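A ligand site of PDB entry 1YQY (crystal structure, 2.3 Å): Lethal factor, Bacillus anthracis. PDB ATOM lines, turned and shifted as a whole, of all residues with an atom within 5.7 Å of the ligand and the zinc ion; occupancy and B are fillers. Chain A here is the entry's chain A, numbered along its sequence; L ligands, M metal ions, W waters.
The side-chain carboxylate (OE1) of Glu 430 sits close to a nitrogen (N2) of the ligand.
N of Gly 400 lies within hydrogen-bond range of O3 of the ligand (3.1 Å).
The backbone carbonyl oxygen of Gly 400 lies within hydrogen-bond range of a nitrogen (N2) of the ligand, at 2.8 Å.
N1 of the ligand sits at hydrogen-bond distance from OH of Tyr 471 (3.0 Å).
OG of Ser 398 lies close to O3 of the ligand, 3.4 Å away.
An oxygen (O3) of the ligand lies within hydrogen-bond range of the backbone NH of Lys 399 (3.2 Å).
ND1 of His 429 is in hydrogen-bond range of OE2 of Glu 482 (2.9 Å).
The side-chain carboxylate of Glu 478 lies close to the side-chain hydroxyl of Tyr 471 (3.4 Å).
OE1 of Glu 430 lies close to N of Leu 401, at 3.4 Å.
The side-chain carboxylate (OE2) of Glu 430 lies within hydrogen-bond range of the backbone NH (N) of Tyr 402, at 3.5 Å.
O of Gly 400 lies within hydrogen-bond range of OG of Ser 398 (2.9 Å).
OH of Tyr 471 is in hydrogen-bond range of OD2 of Asp 71 (3.1 Å).
NH2 of Arg 485 lies within salt-bridge range of OE1 of Glu 482, at 2.6 Å.
Residues that only touch the ligand: Glu 482 (3.4 Å), Leu 420 (3.5 Å), Asp 71 (3.5 Å), Val 418 (3.5 Å), Leu 401 (3.6 Å), Val 396 (3.7 Å), Arg 485 (3.8 Å) and Gly 426 (3.96 Å).
Hydrophobic or aromatic side chains within 4 Å of the ligand: Val 396, Leu 401, Val 418, Leu 420, His 429, His 433 and Tyr 471.
16 residues have an atom within 4 Å of the ligand: Asp 71, Val 396, Ser 398, Lys 399, Gly 400, Leu 401, Val 418, Leu 420, Gly 426, His 429, Glu 430, His 433, Tyr 471, Glu 478, Glu 482 and Arg 485.
The nearest printed residue that does not touch the ligand is Glu 425 (4.2 Å).
Within 4 Å of the zinc ion: His 429, His 433 and Glu 478.
The nearest printed residue that does not touch the zinc ion is Glu 430 (4.2 Å).
The zinc ion is bound by a ring nitrogen (NE2) of His 433 (2.0 Å), a ring nitrogen (NE2) of His 429 (2.1 Å), an oxygen (O2) of the ligand (2.2 Å), the side-chain carboxylate of Glu 478 (2.3 Å) and an oxygen (O1) of the ligand (2.4 Å).
Water W1 lies within hydrogen-bond range of the backbone NH of Tyr 402 (3.3 Å) and a nitrogen (N2) of the ligand (3.4 Å).
Water W2 lies within hydrogen-bond range of O4 of the ligand (3.1 Å), N of Lys 399 (3.1 Å) and O of Lys 416 (3.3 Å).
Water W3 lies within hydrogen-bond range of the backbone carbonyl oxygen (O) of Val 418 (2.6 Å), the side-chain carboxylate (OE1) of Glu 482 (2.8 Å) and the guanidinium group (NH2) of Arg 485 (3.3 Å).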
ATOM      1  N   ASP A  71     -24.390 -19.332  27.606  1.00  0.00           N
ATOM      2  CA  ASP A  71     -24.978 -20.661  27.466  1.00  0.00           C
ATOM      3  C   ASP A  71     -25.971 -20.982  28.590  1.00  0.00           C
ATOM      4  O   ASP A  71     -26.422 -22.134  28.739  1.00  0.00           O
ATOM      5  CB  ASP A  71     -23.870 -21.739  27.452  1.00  0.00           C
ATOM      6  CG  ASP A  71     -22.828 -21.517  28.529  1.00  0.00           C
ATOM      7  OD1 ASP A  71     -22.908 -20.477  29.232  1.00  0.00           O
ATOM      8  OD2 ASP A  71     -21.926 -22.381  28.671  1.00  0.00           O
ATOM      9  N   PHE A  72     -26.296 -19.945  29.372  1.00  0.00           N
ATOM     10  CA  PHE A  72     -27.183 -20.086  30.520  1.00  0.00           C
ATOM     11  C   PHE A  72     -28.437 -19.170  30.470  1.00  0.00           C
ATOM     12  O   PHE A  72     -29.100 -18.947  31.475  1.00  0.00           O
ATOM     13  CB  PHE A  72     -26.390 -19.869  31.802  1.00  0.00           C
ATOM     14  CG  PHE A  72     -25.592 -18.583  31.848  1.00  0.00           C
ATOM     15  CD1 PHE A  72     -26.114 -17.443  32.443  1.00  0.00           C
ATOM     16  CD2 PHE A  72     -24.284 -18.544  31.347  1.00  0.00           C
ATOM     17  CE1 PHE A  72     -25.349 -16.288  32.558  1.00  0.00           C
ATOM     18  CE2 PHE A  72     -23.517 -17.396  31.512  1.00  0.00           C
ATOM     19  CZ  PHE A  72     -24.050 -16.257  32.078  1.00  0.00           C
ATOM     20  N   VAL A 396     -27.901 -22.799  37.343  1.00  0.00           N
ATOM     21  CA  VAL A 396     -27.913 -22.754  35.898  1.00  0.00           C
ATOM     22  C   VAL A 396     -29.000 -23.590  35.287  1.00  0.00           C
ATOM     23  O   VAL A 396     -29.326 -24.662  35.788  1.00  0.00           O
ATOM     24  CB  VAL A 396     -26.548 -23.297  35.326  1.00  0.00           C
ATOM     25  CG1 VAL A 396     -26.648 -23.509  33.909  1.00  0.00           C
ATOM     26  CG2 VAL A 396     -25.409 -22.348  35.609  1.00  0.00           C
ATOM     27  N   HIS A 397     -29.593 -23.084  34.207  1.00  0.00           N
ATOM     28  CA  HIS A 397     -30.543 -23.883  33.431  1.00  0.00           C
ATOM     29  C   HIS A 397     -29.871 -24.044  32.062  1.00  0.00           C
ATOM     30  O   HIS A 397     -29.297 -23.087  31.557  1.00  0.00           O
ATOM     31  CB  HIS A 397     -31.902 -23.234  33.273  1.00  0.00           C
ATOM     32  CG  HIS A 397     -32.775 -23.951  32.292  1.00  0.00           C
ATOM     33  ND1 HIS A 397     -32.931 -25.326  32.275  1.00  0.00           N
ATOM     34  CD2 HIS A 397     -33.460 -23.492  31.209  1.00  0.00           C
ATOM     35  CE1 HIS A 397     -33.718 -25.676  31.274  1.00  0.00           C
ATOM     36  NE2 HIS A 397     -34.043 -24.588  30.601  1.00  0.00           N
ATOM     37  N   SER A 398     -29.851 -25.257  31.527  1.00  0.00           N
ATOM     38  CA  SER A 398     -29.207 -25.495  30.250  1.00  0.00           C
ATOM     39  C   SER A 398     -29.639 -26.880  29.813  1.00  0.00           C
ATOM     40  O   SER A 398     -30.397 -27.525  30.537  1.00  0.00           O
ATOM     41  CB  SER A 398     -27.670 -25.430  30.392  1.00  0.00           C
ATOM     42  OG  SER A 398     -27.184 -26.306  31.432  1.00  0.00           O
ATOM     43  N   LYS A 399     -29.192 -27.312  28.632  1.00  0.00           N
ATOM     44  CA  LYS A 399     -29.507 -28.645  28.122  1.00  0.00           C
ATOM     45  C   LYS A 399     -29.057 -29.717  29.089  1.00  0.00           C
ATOM     46  O   LYS A 399     -29.771 -30.695  29.334  1.00  0.00           O
ATOM     47  CB  LYS A 399     -28.778 -28.907  26.780  1.00  0.00           C
ATOM     48  CG  LYS A 399     -29.062 -30.293  26.136  1.00  0.00           C
ATOM     49  CD  LYS A 399     -30.567 -30.483  26.061  1.00  0.00           C
ATOM     50  CE  LYS A 399     -31.034 -31.213  24.860  1.00  0.00           C
ATOM     51  NZ  LYS A 399     -32.534 -31.295  24.853  1.00  0.00           N
ATOM     52  N   GLY A 400     -27.817 -29.602  29.555  1.00  0.00           N
ATOM     53  CA  GLY A 400     -27.244 -30.645  30.400  1.00  0.00           C
ATOM     54  C   GLY A 400     -26.387 -30.064  31.508  1.00  0.00           C
ATOM     55  O   GLY A 400     -25.935 -28.919  31.409  1.00  0.00           O
ATOM     56  N   LEU A 401     -26.153 -30.880  32.528  1.00  0.00           N
ATOM     57  CA  LEU A 401     -25.285 -30.500  33.637  1.00  0.00           C
ATOM     58  C   LEU A 401     -24.727 -31.714  34.390  1.00  0.00           C
ATOM     59  O   LEU A 401     -25.428 -32.720  34.583  1.00  0.00           O
ATOM     60  CB  LEU A 401     -26.067 -29.583  34.617  1.00  0.00           C
ATOM     61  CG  LEU A 401     -25.296 -28.715  35.603  1.00  0.00           C
ATOM     62  CD1 LEU A 401     -24.401 -27.691  34.882  1.00  0.00           C
ATOM     63  CD2 LEU A 401     -26.247 -28.000  36.492  1.00  0.00           C
ATOM     64  N   TYR A 402     -23.472 -31.629  34.813  1.00  0.00           N
ATOM     65  CA  TYR A 402     -22.902 -32.647  35.676  1.00  0.00           C
ATOM     66  C   TYR A 402     -22.601 -31.919  37.003  1.00  0.00           C
ATOM     67  O   TYR A 402     -21.910 -30.883  37.008  1.00  0.00           O
ATOM     68  CB  TYR A 402     -21.614 -33.217  35.144  1.00  0.00           C
ATOM     69  CG  TYR A 402     -21.003 -34.206  36.142  1.00  0.00           C
ATOM     70  CD1 TYR A 402     -21.635 -35.412  36.429  1.00  0.00           C
ATOM     71  CD2 TYR A 402     -19.881 -33.876  36.873  1.00  0.00           C
ATOM     72  CE1 TYR A 402     -21.124 -36.283  37.392  1.00  0.00           C
ATOM     73  CE2 TYR A 402     -19.329 -34.768  37.780  1.00  0.00           C
ATOM     74  CZ  TYR A 402     -19.986 -35.933  38.062  1.00  0.00           C
ATOM     75  OH  TYR A 402     -19.530 -36.721  39.035  1.00  0.00           O
ATOM     76  N   LYS A 416     -32.421 -26.947  23.674  1.00  0.00           N
ATOM     77  CA  LYS A 416     -31.505 -27.255  22.599  1.00  0.00           C
ATOM     78  C   LYS A 416     -30.092 -27.008  23.115  1.00  0.00           C
ATOM     79  O   LYS A 416     -29.841 -26.053  23.827  1.00  0.00           O
ATOM     80  CB  LYS A 416     -31.819 -26.329  21.401  1.00  0.00           C
ATOM     81  CG  LYS A 416     -31.057 -26.658  20.130  1.00  0.00           C
ATOM     82  CD  LYS A 416     -31.865 -27.571  19.224  1.00  0.00           C
ATOM     83  CE  LYS A 416     -30.991 -28.174  18.126  1.00  0.00           C
ATOM     84  NZ  LYS A 416     -31.807 -28.926  17.125  1.00  0.00           N
ATOM     85  N   GLY A 417     -29.199 -27.949  22.842  1.00  0.00           N
ATOM     86  CA  GLY A 417     -27.821 -27.804  23.298  1.00  0.00           C
ATOM     87  C   GLY A 417     -27.025 -27.229  22.140  1.00  0.00           C
ATOM     88  O   GLY A 417     -27.470 -27.258  20.993  1.00  0.00           O
ATOM     89  N   VAL A 418     -25.853 -26.703  22.459  1.00  0.00           N
ATOM     90  CA  VAL A 418     -24.963 -26.090  21.470  1.00  0.00           C
ATOM     91  C   VAL A 418     -24.395 -27.104  20.466  1.00  0.00           C
ATOM     92  O   VAL A 418     -23.515 -27.916  20.804  1.00  0.00           O
ATOM     93  CB  VAL A 418     -23.761 -25.401  22.179  1.00  0.00           C
ATOM     94  CG1 VAL A 418     -22.844 -24.755  21.172  1.00  0.00           C
ATOM     95  CG2 VAL A 418     -24.273 -24.365  23.198  1.00  0.00           C
ATOM     96  N   LEU A 420     -25.598 -29.798  18.913  1.00  0.00           N
ATOM     97  CA  LEU A 420     -25.800 -31.203  19.203  1.00  0.00           C
ATOM     98  C   LEU A 420     -26.814 -31.716  18.195  1.00  0.00           C
ATOM     99  O   LEU A 420     -27.664 -30.996  17.755  1.00  0.00           O
ATOM    100  CB  LEU A 420     -26.331 -31.382  20.627  1.00  0.00           C
ATOM    101  CG  LEU A 420     -25.416 -31.065  21.805  1.00  0.00           C
ATOM    102  CD1 LEU A 420     -26.086 -31.524  23.114  1.00  0.00           C
ATOM    103  CD2 LEU A 420     -24.066 -31.707  21.641  1.00  0.00           C
ATOM    104  N   GLU A 425     -26.189 -37.285  22.544  1.00  0.00           N
ATOM    105  CA  GLU A 425     -24.890 -36.618  22.485  1.00  0.00           C
ATOM    106  C   GLU A 425     -24.676 -35.721  23.683  1.00  0.00           C
ATOM    107  O   GLU A 425     -23.586 -35.688  24.252  1.00  0.00           O
ATOM    108  CB  GLU A 425     -24.738 -35.865  21.173  1.00  0.00           C
ATOM    109  CG  GLU A 425     -24.702 -36.755  19.938  1.00  0.00           C
ATOM    110  CD  GLU A 425     -24.224 -35.998  18.710  1.00  0.00           C
ATOM    111  OE1 GLU A 425     -24.650 -34.818  18.530  1.00  0.00           O
ATOM    112  OE2 GLU A 425     -23.385 -36.559  17.964  1.00  0.00           O
ATOM    113  N   GLY A 426     -25.738 -35.049  24.122  1.00  0.00           N
ATOM    114  CA  GLY A 426     -25.628 -34.204  25.327  1.00  0.00           C
ATOM    115  C   GLY A 426     -25.258 -35.069  26.508  1.00  0.00           C
ATOM    116  O   GLY A 426     -24.346 -34.751  27.288  1.00  0.00           O
ATOM    117  N   HIS A 429     -21.590 -36.212  26.529  1.00  0.00           N
ATOM    118  CA  HIS A 429     -20.797 -35.062  26.940  1.00  0.00           C
ATOM    119  C   HIS A 429     -20.869 -34.939  28.443  1.00  0.00           C
ATOM    120  O   HIS A 429     -19.845 -34.775  29.079  1.00  0.00           O
ATOM    121  CB  HIS A 429     -21.334 -33.763  26.267  1.00  0.00           C
ATOM    122  CG  HIS A 429     -20.892 -32.497  26.945  1.00  0.00           C
ATOM    123  ND1 HIS A 429     -20.075 -31.579  26.329  1.00  0.00           N
ATOM    124  CD2 HIS A 429     -21.221 -31.966  28.149  1.00  0.00           C
ATOM    125  CE1 HIS A 429     -19.889 -30.545  27.136  1.00  0.00           C
ATOM    126  NE2 HIS A 429     -20.604 -30.733  28.227  1.00  0.00           N
ATOM    127  N   GLU A 430     -22.053 -35.107  29.034  1.00  0.00           N
ATOM    128  CA  GLU A 430     -22.185 -35.025  30.507  1.00  0.00           C
ATOM    129  C   GLU A 430     -21.379 -36.150  31.150  1.00  0.00           C
ATOM    130  O   GLU A 430     -20.701 -35.955  32.144  1.00  0.00           O
ATOM    131  CB  GLU A 430     -23.654 -35.132  30.949  1.00  0.00           C
ATOM    132  CG  GLU A 430     -24.603 -33.980  30.656  1.00  0.00           C
ATOM    133  CD  GLU A 430     -23.938 -32.604  30.583  1.00  0.00           C
ATOM    134  OE1 GLU A 430     -24.377 -31.842  29.736  1.00  0.00           O
ATOM    135  OE2 GLU A 430     -23.103 -32.231  31.434  1.00  0.00           O
ATOM    136  N   HIS A 433     -17.903 -35.405  31.739  1.00  0.00           N
ATOM    137  CA  HIS A 433     -17.634 -34.691  32.964  1.00  0.00           C
ATOM    138  C   HIS A 433     -17.448 -35.624  34.123  1.00  0.00           C
ATOM    139  O   HIS A 433     -16.617 -35.383  34.984  1.00  0.00           O
ATOM    140  CB  HIS A 433     -18.772 -33.634  33.315  1.00  0.00           C
ATOM    141  CG  HIS A 433     -18.802 -32.447  32.398  1.00  0.00           C
ATOM    142  ND1 HIS A 433     -17.706 -31.649  32.159  1.00  0.00           N
ATOM    143  CD2 HIS A 433     -19.791 -31.956  31.614  1.00  0.00           C
ATOM    144  CE1 HIS A 433     -18.022 -30.713  31.289  1.00  0.00           C
ATOM    145  NE2 HIS A 433     -19.285 -30.875  30.943  1.00  0.00           N
ATOM    146  N   TYR A 471     -17.627 -24.516  21.324  1.00  0.00           N
ATOM    147  CA  TYR A 471     -17.983 -24.770  22.716  1.00  0.00           C
ATOM    148  C   TYR A 471     -16.837 -25.426  23.502  1.00  0.00           C
ATOM    149  O   TYR A 471     -16.680 -25.203  24.711  1.00  0.00           O
ATOM    150  CB  TYR A 471     -19.287 -25.573  22.826  1.00  0.00           C
ATOM    151  CG  TYR A 471     -19.851 -25.570  24.219  1.00  0.00           C
ATOM    152  CD1 TYR A 471     -20.387 -24.402  24.761  1.00  0.00           C
ATOM    153  CD2 TYR A 471     -19.669 -26.668  25.064  1.00  0.00           C
ATOM    154  CE1 TYR A 471     -20.798 -24.348  26.083  1.00  0.00           C
ATOM    155  CE2 TYR A 471     -20.066 -26.599  26.398  1.00  0.00           C
ATOM    156  CZ  TYR A 471     -20.636 -25.440  26.892  1.00  0.00           C
ATOM    157  OH  TYR A 471     -21.005 -25.352  28.204  1.00  0.00           O
ATOM    158  N   GLU A 478     -14.898 -28.284  29.869  1.00  0.00           N
ATOM    159  CA  GLU A 478     -15.753 -28.424  28.691  1.00  0.00           C
ATOM    160  C   GLU A 478     -15.023 -28.954  27.472  1.00  0.00           C
ATOM    161  O   GLU A 478     -15.616 -29.615  26.596  1.00  0.00           O
ATOM    162  CB  GLU A 478     -16.365 -27.073  28.308  1.00  0.00           C
ATOM    163  CG  GLU A 478     -17.014 -26.362  29.473  1.00  0.00           C
ATOM    164  CD  GLU A 478     -18.201 -27.133  29.999  1.00  0.00           C
ATOM    165  OE1 GLU A 478     -18.851 -27.825  29.190  1.00  0.00           O
ATOM    166  OE2 GLU A 478     -18.394 -27.151  31.228  1.00  0.00           O
ATOM    167  N   ALA A 481     -14.754 -32.580  27.946  1.00  0.00           N
ATOM    168  CA  ALA A 481     -16.074 -33.195  27.782  1.00  0.00           C
ATOM    169  C   ALA A 481     -16.471 -33.278  26.308  1.00  0.00           C
ATOM    170  O   ALA A 481     -17.059 -34.258  25.866  1.00  0.00           O
ATOM    171  CB  ALA A 481     -17.113 -32.454  28.622  1.00  0.00           C
ATOM    172  N   GLU A 482     -16.174 -32.219  25.568  1.00  0.00           N
ATOM    173  CA  GLU A 482     -16.453 -32.140  24.111  1.00  0.00           C
ATOM    174  C   GLU A 482     -15.596 -33.126  23.288  1.00  0.00           C
ATOM    175  O   GLU A 482     -16.077 -33.809  22.385  1.00  0.00           O
ATOM    176  CB  GLU A 482     -16.208 -30.701  23.601  1.00  0.00           C
ATOM    177  CG  GLU A 482     -17.408 -29.752  23.790  1.00  0.00           C
ATOM    178  CD  GLU A 482     -18.659 -30.256  23.105  1.00  0.00           C
ATOM    179  OE1 GLU A 482     -19.050 -29.672  22.078  1.00  0.00           O
ATOM    180  OE2 GLU A 482     -19.247 -31.260  23.580  1.00  0.00           O
ATOM    181  N   ARG A 485     -16.912 -36.508  24.021  1.00  0.00           N
ATOM    182  CA  ARG A 485     -18.147 -36.739  23.284  1.00  0.00           C
ATOM    183  C   ARG A 485     -17.865 -37.091  21.840  1.00  0.00           C
ATOM    184  O   ARG A 485     -18.526 -37.971  21.260  1.00  0.00           O
ATOM    185  CB  ARG A 485     -18.997 -35.468  23.274  1.00  0.00           C
ATOM    186  CG  ARG A 485     -20.132 -35.529  22.277  1.00  0.00           C
ATOM    187  CD  ARG A 485     -21.113 -34.363  22.466  1.00  0.00           C
ATOM    188  NE  ARG A 485     -20.562 -33.087  22.034  1.00  0.00           N
ATOM    189  CZ  ARG A 485     -20.581 -32.636  20.764  1.00  0.00           C
ATOM    190  NH1 ARG A 485     -21.093 -33.387  19.788  1.00  0.00           N
ATOM    191  NH2 ARG A 485     -20.134 -31.393  20.481  1.00  0.00           N
HETATM  192  C1  LIG L   1     -24.299 -28.288  26.710  1.00  0.00           C
HETATM  193  C2  LIG L   1     -23.414 -28.090  25.598  1.00  0.00           C
HETATM  194  C3  LIG L   1     -22.850 -29.216  24.956  1.00  0.00           C
HETATM  195  C4  LIG L   1     -23.186 -30.497  25.449  1.00  0.00           C
HETATM  196  C5  LIG L   1     -24.042 -30.706  26.595  1.00  0.00           C
HETATM  197  C6  LIG L   1     -24.600 -29.591  27.202  1.00  0.00           C
HETATM  198  F1  LIG L   1     -22.701 -31.586  24.832  1.00  0.00           F
HETATM  199  C7  LIG L   1     -21.956 -29.050  23.750  1.00  0.00           C
HETATM  200  S1  LIG L   1     -25.068 -26.883  27.462  1.00  0.00           S
HETATM  201  N1  LIG L   1     -23.877 -26.086  28.442  1.00  0.00           N
HETATM  202  C8  LIG L   1     -23.674 -26.539  29.821  1.00  0.00           C
HETATM  203  C9  LIG L   1     -22.758 -27.781  29.930  1.00  0.00           C
HETATM  204  N2  LIG L   1     -23.239 -28.764  30.747  1.00  0.00           N
HETATM  205  O1  LIG L   1     -22.471 -29.904  30.921  1.00  0.00           O
HETATM  206  O2  LIG L   1     -21.703 -27.881  29.372  1.00  0.00           O
HETATM  207  O3  LIG L   1     -25.969 -27.322  28.465  1.00  0.00           O
HETATM  208  O4  LIG L   1     -25.459 -25.949  26.418  1.00  0.00           O
HETATM  209  C10 LIG L   1     -23.075 -25.493  30.770  1.00  0.00           C
HETATM  210  C11 LIG L   1     -23.879 -24.154  30.946  1.00  0.00           C
HETATM  211  C12 LIG L   1     -23.241 -23.146  31.899  1.00  0.00           C
HETATM  212  O5  LIG L   1     -23.015 -23.767  33.148  1.00  0.00           O
HETATM  213  C13 LIG L   1     -22.162 -24.927  33.111  1.00  0.00           C
HETATM  214  C14 LIG L   1     -22.769 -26.007  32.198  1.00  0.00           C
HETATM  215 ZN    ZN M   1     -20.313 -29.479  29.855  1.00  0.00          ZN
HETATM  216  O   HOH W   1     -21.495 -29.221  33.656  1.00  0.00           O
HETATM  217  O   HOH W   2     -28.381 -25.094  26.619  1.00  0.00           O
HETATM  218  O   HOH W   3     -20.917 -28.210  20.617  1.00  0.00           O
